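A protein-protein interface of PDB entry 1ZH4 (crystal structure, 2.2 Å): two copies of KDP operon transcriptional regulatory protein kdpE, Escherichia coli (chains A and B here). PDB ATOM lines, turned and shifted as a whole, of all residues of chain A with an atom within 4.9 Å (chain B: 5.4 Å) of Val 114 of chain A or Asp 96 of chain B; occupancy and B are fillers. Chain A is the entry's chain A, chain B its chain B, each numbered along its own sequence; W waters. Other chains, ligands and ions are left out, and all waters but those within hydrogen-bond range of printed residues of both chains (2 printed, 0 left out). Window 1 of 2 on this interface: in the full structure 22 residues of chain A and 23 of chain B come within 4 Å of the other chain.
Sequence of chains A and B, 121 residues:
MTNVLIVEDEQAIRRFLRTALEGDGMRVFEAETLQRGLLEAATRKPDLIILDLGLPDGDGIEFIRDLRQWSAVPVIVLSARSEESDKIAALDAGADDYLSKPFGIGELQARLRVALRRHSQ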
ATOM      1  N   ALA A 110       7.321   8.324  -3.814  1.00  0.00           N
ATOM      2  CA  ALA A 110       6.946   7.078  -3.078  1.00  0.00           C
ATOM      3  C   ALA A 110       6.862   7.393  -1.599  1.00  0.00           C
ATOM      4  O   ALA A 110       5.971   6.926  -0.931  1.00  0.00           O
ATOM      5  CB  ALA A 110       7.949   5.907  -3.336  1.00  0.00           C
ATOM      6  N   ARG A 111       7.773   8.221  -1.105  1.00  0.00           N
ATOM      7  CA  ARG A 111       7.755   8.701   0.286  1.00  0.00           C
ATOM      8  C   ARG A 111       6.595   9.645   0.611  1.00  0.00           C
ATOM      9  O   ARG A 111       6.094   9.700   1.737  1.00  0.00           O
ATOM     10  CB  ARG A 111       9.110   9.386   0.656  1.00  0.00           C
ATOM     11  CG  ARG A 111      10.337   8.382   0.709  1.00  0.00           C
ATOM     12  CD  ARG A 111      11.711   9.037   0.987  1.00  0.00           C
ATOM     13  NE  ARG A 111      12.742   7.978   1.051  1.00  0.00           N
ATOM     14  CZ  ARG A 111      13.034   7.248   2.125  1.00  0.00           C
ATOM     15  NH1 ARG A 111      12.437   7.482   3.269  1.00  0.00           N
ATOM     16  NH2 ARG A 111      13.975   6.317   2.055  1.00  0.00           N
ATOM     17  N   LEU A 112       6.164  10.399  -0.375  1.00  0.00           N
ATOM     18  CA  LEU A 112       4.959  11.212  -0.217  1.00  0.00           C
ATOM     19  C   LEU A 112       3.793  10.269   0.004  1.00  0.00           C
ATOM     20  O   LEU A 112       2.983  10.465   0.900  1.00  0.00           O
ATOM     21  CB  LEU A 112       4.753  12.014  -1.483  1.00  0.00           C
ATOM     22  CG  LEU A 112       4.867  13.516  -1.413  1.00  0.00           C
ATOM     23  CD1 LEU A 112       6.212  14.039  -0.971  1.00  0.00           C
ATOM     24  CD2 LEU A 112       4.451  14.107  -2.796  1.00  0.00           C
ATOM     25  N   ARG A 113       3.746   9.207  -0.791  1.00  0.00           N
ATOM     26  CA  ARG A 113       2.661   8.240  -0.637  1.00  0.00           C
ATOM     27  C   ARG A 113       2.591   7.592   0.738  1.00  0.00           C
ATOM     28  O   ARG A 113       1.499   7.396   1.294  1.00  0.00           O
ATOM     29  CB  ARG A 113       2.743   7.172  -1.709  1.00  0.00           C
ATOM     30  CG  ARG A 113       2.312   7.668  -3.074  1.00  0.00           C
ATOM     31  CD  ARG A 113       2.205   6.582  -4.126  1.00  0.00           C
ATOM     32  NE  ARG A 113       3.485   6.005  -4.554  1.00  0.00           N
ATOM     33  CZ  ARG A 113       4.176   6.517  -5.548  1.00  0.00           C
ATOM     34  NH1 ARG A 113       3.712   7.613  -6.166  1.00  0.00           N
ATOM     35  NH2 ARG A 113       5.301   5.939  -5.960  1.00  0.00           N
ATOM     36  N   VAL A 114       3.763   7.249   1.305  1.00  0.00           N
ATOM     37  CA  VAL A 114       3.790   6.712   2.670  1.00  0.00           C
ATOM     38  C   VAL A 114       3.121   7.718   3.629  1.00  0.00           C
ATOM     39  O   VAL A 114       2.310   7.345   4.508  1.00  0.00           O
ATOM     40  CB  VAL A 114       5.231   6.508   3.182  1.00  0.00           C
ATOM     41  CG1 VAL A 114       5.223   6.178   4.680  1.00  0.00           C
ATOM     42  CG2 VAL A 114       6.033   5.537   2.294  1.00  0.00           C
ATOM     43  N   ALA A 115       3.464   8.984   3.488  1.00  0.00           N
ATOM     44  CA  ALA A 115       2.954   9.948   4.450  1.00  0.00           C
ATOM     45  C   ALA A 115       1.450  10.119   4.254  1.00  0.00           C
ATOM     46  O   ALA A 115       0.714  10.327   5.237  1.00  0.00           O
ATOM     47  CB  ALA A 115       3.659  11.274   4.313  1.00  0.00           C
ATOM     48  N   LEU A 116       0.969  10.032   3.016  1.00  0.00           N
ATOM     49  CA  LEU A 116      -0.489  10.147   2.836  1.00  0.00           C
ATOM     50  C   LEU A 116      -1.177   8.959   3.463  1.00  0.00           C
ATOM     51  O   LEU A 116      -2.125   9.119   4.279  1.00  0.00           O
ATOM     52  CB  LEU A 116      -0.879  10.250   1.381  1.00  0.00           C
ATOM     53  CG  LEU A 116      -0.285  11.462   0.639  1.00  0.00           C
ATOM     54  CD1 LEU A 116      -0.645  11.363  -0.839  1.00  0.00           C
ATOM     55  CD2 LEU A 116      -0.788  12.771   1.248  1.00  0.00           C
ATOM     56  N   ARG A 117      -0.711   7.748   3.146  1.00  0.00           N
ATOM     57  CA  ARG A 117      -1.442   6.607   3.691  1.00  0.00           C
ATOM     58  C   ARG A 117      -1.424   6.526   5.205  1.00  0.00           C
ATOM     59  O   ARG A 117      -2.408   6.122   5.775  1.00  0.00           O
ATOM     60  CB  ARG A 117      -1.049   5.270   3.039  1.00  0.00           C
ATOM     61  CG  ARG A 117       0.332   4.737   3.339  1.00  0.00           C
ATOM     62  CD  ARG A 117       0.554   3.342   2.739  1.00  0.00           C
ATOM     63  NE  ARG A 117       1.912   2.846   2.991  1.00  0.00           N
ATOM     64  CZ  ARG A 117       2.931   2.966   2.133  1.00  0.00           C
ATOM     65  NH1 ARG A 117       2.768   3.605   0.927  1.00  0.00           N
ATOM     66  NH2 ARG A 117       4.130   2.433   2.477  1.00  0.00           N
ATOM     67  N   ARG A 118      -0.320   6.924   5.852  1.00  0.00           N
ATOM     68  CA  ARG A 118      -0.174   6.799   7.302  1.00  0.00           C
ATOM     69  C   ARG A 118      -0.950   7.867   8.069  1.00  0.00           C
ATOM     70  O   ARG A 118      -1.329   7.637   9.206  1.00  0.00           O
ATOM     71  CB  ARG A 118       1.311   6.818   7.729  1.00  0.00           C
ATOM     72  CG  ARG A 118       2.048   5.462   7.602  1.00  0.00           C
ATOM     73  CD  ARG A 118       1.500   4.385   8.547  1.00  0.00           C
ATOM     74  NE  ARG A 118       2.264   3.155   8.397  1.00  0.00           N
ATOM     75  CZ  ARG A 118       1.948   1.977   8.961  1.00  0.00           C
ATOM     76  NH1 ARG A 118       0.849   1.840   9.711  1.00  0.00           N
ATOM     77  NH2 ARG A 118       2.740   0.923   8.760  1.00  0.00           N
ATOM     78  N   HIS A 119      -1.179   9.024   7.456  1.00  0.00           N
ATOM     79  CA  HIS A 119      -1.979  10.093   8.071  1.00  0.00           C
ATOM     80  C   HIS A 119      -3.464  10.172   7.760  1.00  0.00           C
ATOM     81  O   HIS A 119      -4.170  11.005   8.347  1.00  0.00           O
ATOM     82  CB  HIS A 119      -1.333  11.441   7.792  1.00  0.00           C
ATOM     83  CG  HIS A 119      -0.035  11.571   8.499  1.00  0.00           C
ATOM     84  ND1 HIS A 119       1.122  10.976   8.029  1.00  0.00           N
ATOM     85  CD2 HIS A 119       0.256  12.057   9.730  1.00  0.00           C
ATOM     86  CE1 HIS A 119       2.089  11.170   8.909  1.00  0.00           C
ATOM     87  NE2 HIS A 119       1.593  11.837   9.941  1.00  0.00           N
ATOM     88  N   ARG B  68       1.606  -6.941   5.195  1.00  0.00           N
ATOM     89  CA  ARG B  68       0.528  -5.947   5.082  1.00  0.00           C
ATOM     90  C   ARG B  68      -0.908  -6.492   4.901  1.00  0.00           C
ATOM     91  O   ARG B  68      -1.880  -5.825   5.241  1.00  0.00           O
ATOM     92  CB  ARG B  68       0.916  -4.987   3.949  1.00  0.00           C
ATOM     93  CG  ARG B  68       2.030  -4.044   4.307  1.00  0.00           C
ATOM     94  CD  ARG B  68       1.643  -3.128   5.484  1.00  0.00           C
ATOM     95  NE  ARG B  68       2.734  -2.253   5.908  1.00  0.00           N
ATOM     96  CZ  ARG B  68       3.231  -2.240   7.142  1.00  0.00           C
ATOM     97  NH1 ARG B  68       2.722  -3.055   8.071  1.00  0.00           N
ATOM     98  NH2 ARG B  68       4.231  -1.423   7.441  1.00  0.00           N
ATOM     99  N   ALA B  72      -0.438  -3.803  10.229  1.00  0.00           N
ATOM    100  CA  ALA B  72      -0.076  -2.443   9.900  1.00  0.00           C
ATOM    101  C   ALA B  72       1.155  -1.973  10.681  1.00  0.00           C
ATOM    102  O   ALA B  72       1.391  -0.770  10.737  1.00  0.00           O
ATOM    103  CB  ALA B  72      -1.257  -1.538  10.203  1.00  0.00           C
ATOM    104  N   VAL B  73       1.905  -2.879  11.352  1.00  0.00           N
ATOM    105  CA  VAL B  73       3.094  -2.405  12.127  1.00  0.00           C
ATOM    106  C   VAL B  73       4.102  -1.736  11.223  1.00  0.00           C
ATOM    107  O   VAL B  73       4.329  -2.170  10.111  1.00  0.00           O
ATOM    108  CB  VAL B  73       3.850  -3.558  12.803  1.00  0.00           C
ATOM    109  CG1 VAL B  73       2.990  -4.151  13.834  1.00  0.00           C
ATOM    110  CG2 VAL B  73       4.157  -4.634  11.740  1.00  0.00           C
ATOM    111  N   PRO B  74       4.711  -0.685  11.734  1.00  0.00           N
ATOM    112  CA  PRO B  74       5.734   0.073  11.017  1.00  0.00           C
ATOM    113  C   PRO B  74       6.899  -0.821  10.622  1.00  0.00           C
ATOM    114  O   PRO B  74       7.229  -1.808  11.348  1.00  0.00           O
ATOM    115  CB  PRO B  74       6.144   1.123  12.042  1.00  0.00           C
ATOM    116  CG  PRO B  74       4.889   1.298  12.851  1.00  0.00           C
ATOM    117  CD  PRO B  74       4.458  -0.123  13.080  1.00  0.00           C
ATOM    118  N   VAL B  75       7.451  -0.536   9.439  1.00  0.00           N
ATOM    119  CA  VAL B  75       8.470  -1.385   8.853  1.00  0.00           C
ATOM    120  C   VAL B  75       9.513  -0.476   8.258  1.00  0.00           C
ATOM    121  O   VAL B  75       9.210   0.419   7.441  1.00  0.00           O
ATOM    122  CB  VAL B  75       7.945  -2.340   7.734  1.00  0.00           C
ATOM    123  CG1 VAL B  75       9.167  -3.022   6.938  1.00  0.00           C
ATOM    124  CG2 VAL B  75       7.038  -3.399   8.250  1.00  0.00           C
ATOM    125  N   ILE B  76      10.755  -0.673   8.693  1.00  0.00           N
ATOM    126  CA  ILE B  76      11.854   0.156   8.205  1.00  0.00           C
ATOM    127  C   ILE B  76      12.737  -0.828   7.530  1.00  0.00           C
ATOM    128  O   ILE B  76      13.113  -1.854   8.138  1.00  0.00           O
ATOM    129  CB  ILE B  76      12.555   0.874   9.360  1.00  0.00           C
ATOM    130  CG1 ILE B  76      11.666   2.008   9.854  1.00  0.00           C
ATOM    131  CG2 ILE B  76      13.909   1.449   8.949  1.00  0.00           C
ATOM    132  CD1 ILE B  76      12.270   2.877  10.951  1.00  0.00           C
ATOM    133  N   LEU B  91       8.752   0.761  -0.509  1.00  0.00           N
ATOM    134  CA  LEU B  91       7.822   1.715   0.101  1.00  0.00           C
ATOM    135  C   LEU B  91       6.377   1.516  -0.422  1.00  0.00           C
ATOM    136  O   LEU B  91       5.413   1.589   0.375  1.00  0.00           O
ATOM    137  CB  LEU B  91       8.273   3.168  -0.130  1.00  0.00           C
ATOM    138  CG  LEU B  91       9.641   3.490   0.513  1.00  0.00           C
ATOM    139  CD1 LEU B  91      10.168   4.842   0.043  1.00  0.00           C
ATOM    140  CD2 LEU B  91       9.624   3.507   1.979  1.00  0.00           C
ATOM    141  N   GLY B  94       4.605  -1.308   0.913  1.00  0.00           N
ATOM    142  CA  GLY B  94       4.108  -1.052   2.258  1.00  0.00           C
ATOM    143  C   GLY B  94       5.120  -0.751   3.375  1.00  0.00           C
ATOM    144  O   GLY B  94       4.779  -0.478   4.511  1.00  0.00           O
ATOM    145  N   ALA B  95       6.385  -0.729   3.050  1.00  0.00           N
ATOM    146  CA  ALA B  95       7.353  -0.323   4.067  1.00  0.00           C
ATOM    147  C   ALA B  95       7.126   1.121   4.332  1.00  0.00           C
ATOM    148  O   ALA B  95       6.606   1.870   3.478  1.00  0.00           O
ATOM    149  CB  ALA B  95       8.761  -0.544   3.570  1.00  0.00           C
ATOM    150  N   ASP B  96       7.551   1.541   5.509  1.00  0.00           N
ATOM    151  CA  ASP B  96       7.341   2.874   5.965  1.00  0.00           C
ATOM    152  C   ASP B  96       8.561   3.741   5.748  1.00  0.00           C
ATOM    153  O   ASP B  96       8.456   4.968   5.631  1.00  0.00           O
ATOM    154  CB  ASP B  96       6.978   2.801   7.426  1.00  0.00           C
ATOM    155  CG  ASP B  96       5.583   2.356   7.606  1.00  0.00           C
ATOM    156  OD1 ASP B  96       4.653   3.135   7.367  1.00  0.00           O
ATOM    157  OD2 ASP B  96       5.295   1.183   7.901  1.00  0.00           O
ATOM    158  N   ASP B  97       9.729   3.125   5.683  1.00  0.00           N
ATOM    159  CA  ASP B  97      10.986   3.916   5.557  1.00  0.00           C
ATOM    160  C   ASP B  97      12.042   2.982   5.008  1.00  0.00           C
ATOM    161  O   ASP B  97      11.896   1.767   5.020  1.00  0.00           O
ATOM    162  CB  ASP B  97      11.452   4.528   6.902  1.00  0.00           C
ATOM    163  CG  ASP B  97      12.406   5.719   6.714  1.00  0.00           C
ATOM    164  OD1 ASP B  97      12.945   5.875   5.585  1.00  0.00           O
ATOM    165  OD2 ASP B  97      12.645   6.596   7.594  1.00  0.00           O
ATOM    166  N   TYR B  98      13.133   3.546   4.576  1.00  0.00           N
ATOM    167  CA  TYR B  98      14.147   2.732   3.934  1.00  0.00           C
ATOM    168  C   TYR B  98      15.524   3.370   4.129  1.00  0.00           C
ATOM    169  O   TYR B  98      15.703   4.543   3.809  1.00  0.00           O
ATOM    170  CB  TYR B  98      13.836   2.674   2.450  1.00  0.00           C
ATOM    171  CG  TYR B  98      14.596   1.619   1.656  1.00  0.00           C
ATOM    172  CD1 TYR B  98      15.996   1.645   1.548  1.00  0.00           C
ATOM    173  CD2 TYR B  98      13.927   0.658   0.985  1.00  0.00           C
ATOM    174  CE1 TYR B  98      16.652   0.733   0.800  1.00  0.00           C
ATOM    175  CE2 TYR B  98      14.588  -0.288   0.247  1.00  0.00           C
ATOM    176  CZ  TYR B  98      15.959  -0.233   0.152  1.00  0.00           C
ATOM    177  OH  TYR B  98      16.618  -1.195  -0.613  1.00  0.00           O
HETATM  178  O   HOH W   1       5.003   4.346  -0.984  1.00  0.00           O
HETATM  179  O   HOH W   2       3.403   1.808   5.456  1.00  0.00           O
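Of the 10 printed residues of chain A, 4 touch a printed residue of chain B. Hydrophobic or aromatic side chains of chain A that line the printed part of chain B: Val 114. Of the 12 printed residues of chain B, 10 touch a printed residue of chain A. Hydrophobic or aromatic side chains of chain B that line the printed part of chain A: Leu 91 and Tyr 98. Among the printed residues, Asp or Glu carboxylates within 4 Å of a Lys or Arg side-chain nitrogen of the other chain: Arg 111 of chain A with Asp 97 of chain B (2.9 Å) and Arg 118 of chain A with Asp 96 of chain B (2.6 Å).
NE of Arg 68 of chain B sits at hydrogen-bond distance from O of Gly 94 of chain B. The guanidinium group (NH2) of Arg 68 of chain B lies within salt-bridge range of the side-chain carboxylate (OD2) of Asp 96 of chain B. The backbone carbonyl oxygen (O) of Val 75 of chain B sits at hydrogen-bond distance from the backbone NH (N) of Asp 97 of chain B (3.3 Å). The backbone carbonyl oxygen (O) of Val 75 of chain B sits at hydrogen-bond distance from the backbone NH (N) of Asp 96 of chain B, 2.8 Å away. The backbone carbonyl oxygen (O) of Val 73 of chain B sits at hydrogen-bond distance from the guanidinium group (NH1) of Arg 68 of chain B (2.7 Å).
CG of Arg 111 of chain A touches CD1 of Leu 91 of chain B, 3.6 Å away. O of Ala 95 of chain B touches CG2 of Val 114 of chain A, 3.9 Å away. Asp 96 of chain B touches Val 114 of chain A (O to CG1, 3.6 Å). Gly 94 of chain B touches Arg 117 of chain A. Arg 118 of chain A touches Val 73 of chain B (NH2 to O, 3.7 Å). Pro 74 of chain B touches Arg 118 of chain A (CA to NH2, 3.8 Å).
No position is printed for both chains. Of the 13 pairs that touch across the chains among the printed residues, none has its exchanged pair printed and touching as well.
Of chain B, only Ala 95 and Asp 96 come within 4 Å of Val 114 of chain A. Of the printed residues of chain A, Asp 96 of chain B touches Val 114 and Arg 118. Of the printed residues of chain B, Arg 111 of chain A touches Leu 91 (3.6 Å), Asp 97 (2.9 Å) and Tyr 98 (3.0 Å). Of the printed residues of chain A, Ala 72 of chain B touches Arg 118 (2.9 Å).
Water W2 lies within hydrogen-bond range of the side-chain carboxylate of Asp 96 of chain B, the backbone carbonyl oxygen of Gly 94 of chain B, the guanidinium group of Arg 117 of chain A and the guanidinium group of Arg 118 of chain A. Water W1 lies within hydrogen-bond range of O of Ala 110 of chain A (2.8 Å), NH1 of Arg 117 of chain A (3.0 Å) and O of Leu 91 of chain B (3.1 Å).
The backbone carbonyl oxygen of Tyr 98 of chain B lies within hydrogen-bond range of the guanidinium group of Arg 111 of chain A. NH1 of Arg 118 of chain A lies within hydrogen-bond range of O of Ala 72 of chain B (2.9 Å). The guanidinium group (NH2) of Arg 117 of chain A lies within hydrogen-bond range of the backbone carbonyl oxygen (O) of Ala 95 of chain B (2.7 Å). The guanidinium group (NH2) of Arg 117 of chain A sits at hydrogen-bond distance from the backbone carbonyl oxygen (O) of Leu 91 of chain B. The side-chain carboxylate of Asp 97 of chain B is in salt-bridge range of the guanidinium group of Arg 111 of chain A (2.9 Å). The guanidinium group of Arg 68 of chain B lies close to the guanidinium group of Arg 118 of chain A (3.1 Å). The guanidinium group (NE) of Arg 118 of chain A lies within salt-bridge range of the side-chain carboxylate (OD1) of Asp 96 of chain B.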
